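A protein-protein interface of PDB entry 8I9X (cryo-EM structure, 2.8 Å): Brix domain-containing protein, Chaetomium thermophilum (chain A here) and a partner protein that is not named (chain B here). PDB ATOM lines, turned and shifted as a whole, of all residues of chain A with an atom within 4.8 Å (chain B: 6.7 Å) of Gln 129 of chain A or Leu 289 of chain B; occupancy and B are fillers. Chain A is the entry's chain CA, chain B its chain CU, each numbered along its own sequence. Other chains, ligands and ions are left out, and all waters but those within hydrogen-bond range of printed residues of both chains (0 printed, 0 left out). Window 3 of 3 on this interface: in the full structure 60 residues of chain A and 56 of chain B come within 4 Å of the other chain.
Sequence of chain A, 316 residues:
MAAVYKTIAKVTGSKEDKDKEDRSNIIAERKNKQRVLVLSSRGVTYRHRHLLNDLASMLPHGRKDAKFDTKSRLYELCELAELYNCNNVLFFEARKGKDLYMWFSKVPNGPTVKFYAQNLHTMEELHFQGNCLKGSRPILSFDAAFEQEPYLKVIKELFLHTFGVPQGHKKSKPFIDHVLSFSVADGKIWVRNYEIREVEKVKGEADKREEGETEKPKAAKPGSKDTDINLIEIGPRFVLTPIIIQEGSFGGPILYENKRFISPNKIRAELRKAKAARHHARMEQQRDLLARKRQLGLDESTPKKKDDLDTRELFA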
ATOM      1  N   HIS A 127      34.565  11.022  20.222  1.00  0.00           N
ATOM      2  CA  HIS A 127      34.126   9.903  19.363  1.00  0.00           C
ATOM      3  C   HIS A 127      34.316   8.610  20.125  1.00  0.00           C
ATOM      4  O   HIS A 127      34.041   7.552  19.545  1.00  0.00           O
ATOM      5  CB  HIS A 127      34.956   9.857  18.079  1.00  0.00           C
ATOM      6  CG  HIS A 127      36.431   9.755  18.249  1.00  0.00           C
ATOM      7  ND1 HIS A 127      37.089   8.546  18.268  1.00  0.00           N
ATOM      8  CD2 HIS A 127      37.382  10.706  18.344  1.00  0.00           C
ATOM      9  CE1 HIS A 127      38.381   8.754  18.398  1.00  0.00           C
ATOM     10  NE2 HIS A 127      38.587  10.068  18.450  1.00  0.00           N
ATOM     11  N   PHE A 128      34.759   8.689  21.371  1.00  0.00           N
ATOM     12  CA  PHE A 128      35.126   7.431  22.063  1.00  0.00           C
ATOM     13  C   PHE A 128      33.888   6.703  22.588  1.00  0.00           C
ATOM     14  O   PHE A 128      33.778   5.521  22.213  1.00  0.00           O
ATOM     15  CB  PHE A 128      36.236   7.690  23.075  1.00  0.00           C
ATOM     16  CG  PHE A 128      37.608   7.739  22.456  1.00  0.00           C
ATOM     17  CD1 PHE A 128      38.023   6.745  21.587  1.00  0.00           C
ATOM     18  CD2 PHE A 128      38.485   8.773  22.733  1.00  0.00           C
ATOM     19  CE1 PHE A 128      39.279   6.786  21.006  1.00  0.00           C
ATOM     20  CE2 PHE A 128      39.741   8.810  22.151  1.00  0.00           C
ATOM     21  CZ  PHE A 128      40.138   7.817  21.290  1.00  0.00           C
ATOM     22  N   GLN A 129      33.055   7.324  23.409  1.00  0.00           N
ATOM     23  CA  GLN A 129      31.766   6.707  23.856  1.00  0.00           C
ATOM     24  C   GLN A 129      31.954   5.776  25.059  1.00  0.00           C
ATOM     25  O   GLN A 129      30.947   5.408  25.661  1.00  0.00           O
ATOM     26  CB  GLN A 129      31.010   5.987  22.732  1.00  0.00           C
ATOM     27  CG  GLN A 129      30.309   6.908  21.752  1.00  0.00           C
ATOM     28  CD  GLN A 129      29.373   6.124  20.868  1.00  0.00           C
ATOM     29  OE1 GLN A 129      28.813   5.109  21.273  1.00  0.00           O
ATOM     30  NE2 GLN A 129      29.197   6.595  19.646  1.00  0.00           N
ATOM     31  N   GLY A 130      33.178   5.404  25.400  1.00  0.00           N
ATOM     32  CA  GLY A 130      33.394   4.471  26.518  1.00  0.00           C
ATOM     33  C   GLY A 130      34.050   5.131  27.712  1.00  0.00           C
ATOM     34  O   GLY A 130      34.810   6.073  27.507  1.00  0.00           O
ATOM     35  N   ASN A 131      33.800   4.633  28.920  1.00  0.00           N
ATOM     36  CA  ASN A 131      34.390   5.203  30.150  1.00  0.00           C
ATOM     37  C   ASN A 131      34.647   4.071  31.127  1.00  0.00           C
ATOM     38  O   ASN A 131      34.012   3.024  30.983  1.00  0.00           O
ATOM     39  CB  ASN A 131      33.458   6.234  30.770  1.00  0.00           C
ATOM     40  CG  ASN A 131      34.106   7.164  31.766  1.00  0.00           C
ATOM     41  OD1 ASN A 131      35.292   7.057  32.058  1.00  0.00           O
ATOM     42  ND2 ASN A 131      33.322   8.091  32.284  1.00  0.00           N
ATOM     43  N   ILE A 232      33.643  -1.343  24.099  1.00  0.00           N
ATOM     44  CA  ILE A 232      33.491   0.024  23.613  1.00  0.00           C
ATOM     45  C   ILE A 232      34.774   0.788  23.902  1.00  0.00           C
ATOM     46  O   ILE A 232      35.168   0.912  25.061  1.00  0.00           O
ATOM     47  CB  ILE A 232      32.289   0.729  24.266  1.00  0.00           C
ATOM     48  CG1 ILE A 232      30.983   0.066  23.832  1.00  0.00           C
ATOM     49  CG2 ILE A 232      32.280   2.203  23.906  1.00  0.00           C
ATOM     50  CD1 ILE A 232      29.921   0.061  24.905  1.00  0.00           C
ATOM     51  N   GLU A 233      35.419   1.310  22.862  1.00  0.00           N
ATOM     52  CA  GLU A 233      36.701   1.981  23.056  1.00  0.00           C
ATOM     53  C   GLU A 233      36.525   3.224  23.925  1.00  0.00           C
ATOM     54  O   GLU A 233      35.573   3.986  23.756  1.00  0.00           O
ATOM     55  CB  GLU A 233      37.313   2.348  21.706  1.00  0.00           C
ATOM     56  CG  GLU A 233      38.596   3.147  21.799  1.00  0.00           C
ATOM     57  CD  GLU A 233      39.475   2.972  20.580  1.00  0.00           C
ATOM     58  OE1 GLU A 233      39.211   2.046  19.786  1.00  0.00           O
ATOM     59  OE2 GLU A 233      40.430   3.759  20.416  1.00  0.00           O
ATOM     60  N   ARG B 277      37.052   9.497  32.724  1.00  0.00           N
ATOM     61  CA  ARG B 277      36.465  10.566  31.932  1.00  0.00           C
ATOM     62  C   ARG B 277      35.299  11.167  32.703  1.00  0.00           C
ATOM     63  O   ARG B 277      34.489  10.435  33.280  1.00  0.00           O
ATOM     64  CB  ARG B 277      36.002  10.048  30.574  1.00  0.00           C
ATOM     65  CG  ARG B 277      37.102   9.448  29.723  1.00  0.00           C
ATOM     66  CD  ARG B 277      36.514   8.747  28.517  1.00  0.00           C
ATOM     67  NE  ARG B 277      36.237   9.678  27.430  1.00  0.00           N
ATOM     68  CZ  ARG B 277      35.448   9.412  26.400  1.00  0.00           C
ATOM     69  NH1 ARG B 277      34.837   8.246  26.280  1.00  0.00           N
ATOM     70  NH2 ARG B 277      35.266  10.341  25.466  1.00  0.00           N
ATOM     71  N   MET B 282      31.216  12.907  29.305  1.00  0.00           N
ATOM     72  CA  MET B 282      30.095  12.052  28.926  1.00  0.00           C
ATOM     73  C   MET B 282      28.886  12.845  28.462  1.00  0.00           C
ATOM     74  O   MET B 282      28.199  12.411  27.531  1.00  0.00           O
ATOM     75  CB  MET B 282      29.721  11.128  30.084  1.00  0.00           C
ATOM     76  CG  MET B 282      30.840  10.204  30.476  1.00  0.00           C
ATOM     77  SD  MET B 282      31.292   9.259  29.008  1.00  0.00           S
ATOM     78  CE  MET B 282      33.036   9.578  28.893  1.00  0.00           C
ATOM     79  N   LYS B 284      28.992  15.765  26.873  1.00  0.00           N
ATOM     80  CA  LYS B 284      29.273  16.202  25.504  1.00  0.00           C
ATOM     81  C   LYS B 284      29.172  15.057  24.501  1.00  0.00           C
ATOM     82  O   LYS B 284      28.663  15.256  23.391  1.00  0.00           O
ATOM     83  CB  LYS B 284      30.644  16.873  25.412  1.00  0.00           C
ATOM     84  CG  LYS B 284      31.018  17.719  26.603  1.00  0.00           C
ATOM     85  CD  LYS B 284      32.137  18.684  26.268  1.00  0.00           C
ATOM     86  CE  LYS B 284      32.961  19.014  27.501  1.00  0.00           C
ATOM     87  NZ  LYS B 284      33.861  20.178  27.273  1.00  0.00           N
ATOM     88  N   VAL B 285      29.656  13.865  24.858  1.00  0.00           N
ATOM     89  CA  VAL B 285      29.494  12.717  23.965  1.00  0.00           C
ATOM     90  C   VAL B 285      28.018  12.424  23.730  1.00  0.00           C
ATOM     91  O   VAL B 285      27.586  12.204  22.588  1.00  0.00           O
ATOM     92  CB  VAL B 285      30.232  11.484  24.518  1.00  0.00           C
ATOM     93  CG1 VAL B 285      30.191  10.355  23.506  1.00  0.00           C
ATOM     94  CG2 VAL B 285      31.671  11.825  24.837  1.00  0.00           C
ATOM     95  N   LYS B 286      27.224  12.432  24.803  1.00  0.00           N
ATOM     96  CA  LYS B 286      25.788  12.224  24.679  1.00  0.00           C
ATOM     97  C   LYS B 286      25.160  13.274  23.776  1.00  0.00           C
ATOM     98  O   LYS B 286      24.322  12.957  22.929  1.00  0.00           O
ATOM     99  CB  LYS B 286      25.144  12.251  26.066  1.00  0.00           C
ATOM    100  CG  LYS B 286      23.662  11.940  26.088  1.00  0.00           C
ATOM    101  CD  LYS B 286      23.139  11.912  27.515  1.00  0.00           C
ATOM    102  CE  LYS B 286      21.653  11.610  27.555  1.00  0.00           C
ATOM    103  NZ  LYS B 286      21.132  11.583  28.950  1.00  0.00           N
ATOM    104  N   GLN B 287      25.564  14.535  23.938  1.00  0.00           N
ATOM    105  CA  GLN B 287      24.958  15.611  23.164  1.00  0.00           C
ATOM    106  C   GLN B 287      25.313  15.509  21.687  1.00  0.00           C
ATOM    107  O   GLN B 287      24.477  15.800  20.824  1.00  0.00           O
ATOM    108  CB  GLN B 287      25.373  16.970  23.727  1.00  0.00           C
ATOM    109  CG  GLN B 287      24.804  17.292  25.106  1.00  0.00           C
ATOM    110  CD  GLN B 287      23.288  17.184  25.183  1.00  0.00           C
ATOM    111  OE1 GLN B 287      22.587  17.303  24.179  1.00  0.00           O
ATOM    112  NE2 GLN B 287      22.779  16.955  26.387  1.00  0.00           N
ATOM    113  N   LYS B 288      26.545  15.108  21.367  1.00  0.00           N
ATOM    114  CA  LYS B 288      26.879  14.951  19.955  1.00  0.00           C
ATOM    115  C   LYS B 288      26.142  13.762  19.354  1.00  0.00           C
ATOM    116  O   LYS B 288      25.716  13.804  18.193  1.00  0.00           O
ATOM    117  CB  LYS B 288      28.384  14.820  19.735  1.00  0.00           C
ATOM    118  CG  LYS B 288      28.726  15.094  18.268  1.00  0.00           C
ATOM    119  CD  LYS B 288      30.204  15.123  17.965  1.00  0.00           C
ATOM    120  CE  LYS B 288      30.867  13.854  18.407  1.00  0.00           C
ATOM    121  NZ  LYS B 288      30.934  12.845  17.313  1.00  0.00           N
ATOM    122  N   LEU B 289      25.961  12.693  20.135  1.00  0.00           N
ATOM    123  CA  LEU B 289      25.122  11.598  19.661  1.00  0.00           C
ATOM    124  C   LEU B 289      23.700  12.077  19.392  1.00  0.00           C
ATOM    125  O   LEU B 289      23.095  11.729  18.367  1.00  0.00           O
ATOM    126  CB  LEU B 289      25.117  10.456  20.677  1.00  0.00           C
ATOM    127  CG  LEU B 289      26.349   9.555  20.711  1.00  0.00           C
ATOM    128  CD1 LEU B 289      26.391   8.752  21.999  1.00  0.00           C
ATOM    129  CD2 LEU B 289      26.355   8.639  19.506  1.00  0.00           C
ATOM    130  N   ILE B 290      23.161  12.894  20.300  1.00  0.00           N
ATOM    131  CA  ILE B 290      21.812  13.428  20.137  1.00  0.00           C
ATOM    132  C   ILE B 290      21.718  14.258  18.866  1.00  0.00           C
ATOM    133  O   ILE B 290      20.769  14.119  18.089  1.00  0.00           O
ATOM    134  CB  ILE B 290      21.401  14.253  21.371  1.00  0.00           C
ATOM    135  CG1 ILE B 290      21.337  13.374  22.617  1.00  0.00           C
ATOM    136  CG2 ILE B 290      20.064  14.940  21.135  1.00  0.00           C
ATOM    137  CD1 ILE B 290      20.280  12.319  22.548  1.00  0.00           C
ATOM    138  N   GLU B 291      22.695  15.137  18.635  1.00  0.00           N
ATOM    139  CA  GLU B 291      22.607  16.017  17.474  1.00  0.00           C
ATOM    140  C   GLU B 291      22.775  15.237  16.175  1.00  0.00           C
ATOM    141  O   GLU B 291      22.115  15.543  15.177  1.00  0.00           O
ATOM    142  CB  GLU B 291      23.624  17.156  17.571  1.00  0.00           C
ATOM    143  CG  GLU B 291      25.080  16.757  17.507  1.00  0.00           C
ATOM    144  CD  GLU B 291      26.010  17.947  17.657  1.00  0.00           C
ATOM    145  OE1 GLU B 291      25.506  19.076  17.831  1.00  0.00           O
ATOM    146  OE2 GLU B 291      27.242  17.757  17.596  1.00  0.00           O
ATOM    147  N   GLU B 292      23.638  14.216  16.166  1.00  0.00           N
ATOM    148  CA  GLU B 292      23.783  13.397  14.967  1.00  0.00           C
ATOM    149  C   GLU B 292      22.493  12.650  14.642  1.00  0.00           C
ATOM    150  O   GLU B 292      22.022  12.670  13.492  1.00  0.00           O
ATOM    151  CB  GLU B 292      24.941  12.415  15.143  1.00  0.00           C
ATOM    152  CG  GLU B 292      26.258  12.895  14.559  1.00  0.00           C
ATOM    153  CD  GLU B 292      27.392  11.913  14.785  1.00  0.00           C
ATOM    154  OE1 GLU B 292      27.186  10.923  15.519  1.00  0.00           O
ATOM    155  OE2 GLU B 292      28.488  12.131  14.229  1.00  0.00           O
ATOM    156  N   ALA B 293      21.899  11.993  15.644  1.00  0.00           N
ATOM    157  CA  ALA B 293      20.646  11.283  15.411  1.00  0.00           C
ATOM    158  C   ALA B 293      19.534  12.245  15.009  1.00  0.00           C
ATOM    159  O   ALA B 293      18.713  11.928  14.135  1.00  0.00           O
ATOM    160  CB  ALA B 293      20.249  10.493  16.657  1.00  0.00           C
ATOM    161  N   THR B 294      19.490  13.423  15.636  1.00  0.00           N
ATOM    162  CA  THR B 294      18.484  14.418  15.294  1.00  0.00           C
ATOM    163  C   THR B 294      18.644  14.885  13.856  1.00  0.00           C
ATOM    164  O   THR B 294      17.653  15.037  13.138  1.00  0.00           O
ATOM    165  CB  THR B 294      18.572  15.604  16.257  1.00  0.00           C
ATOM    166  OG1 THR B 294      18.294  15.161  17.590  1.00  0.00           O
ATOM    167  CG2 THR B 294      17.575  16.681  15.873  1.00  0.00           C
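The backbone carbonyl oxygen of Arg 277 of chain B is in hydrogen-bond range of the side-chain amide nitrogen of Asn 131 of chain A (2.8 Å). The backbone carbonyl oxygen (O) of Gly 130 of chain A sits at hydrogen-bond distance from the guanidinium group (NH1) of Arg 277 of chain B, at 2.5 Å.
The backbone carbonyl oxygen (O) of Glu 233 of chain A lies within hydrogen-bond range of the backbone NH (N) of Gly 130 of chain A.
Among the printed residues, pairs that only touch across the chains: Gln 129 of chain A with Arg 277 of chain B (3.5 Å), Gln 129 of chain A with Leu 289 of chain B (3.5 Å), Phe 128 of chain A with Arg 277 of chain B (3.5 Å), Asn 131 of chain A with Met 282 of chain B (3.7 Å) and Gln 129 of chain A with Val 285 of chain B (3.9 Å).
Printed residues of chain B within 4 Å of Phe 128 of chain A: Arg 277 (3.5 Å). Gln 129 of chain A touches just these residues of chain B: Arg 277 (3.5 Å), Val 285 (3.9 Å) and Leu 289 (3.5 Å). Printed residues of chain B within 4 Å of Asn 131 of chain A: Arg 277 (2.8 Å) and Met 282 (3.7 Å). Gln 287 of chain B touches none of the printed residues of chain A. Glu 292 of chain B touches none of the printed residues of chain A. The nearest printed residue of chain A that does not touch Leu 289 of chain B is His 127 of chain A (7.8 Å). The nearest printed residue of chain B that does not touch Gly 130 of chain A is Met 282 of chain B (4.2 Å).
Hydrophobic or aromatic side chains of chain A that line the printed part of chain B: Phe 128. Among the printed residues, no Asp or Glu carboxylate lies within 4 Å of a Lys or Arg side-chain nitrogen of the other chain.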
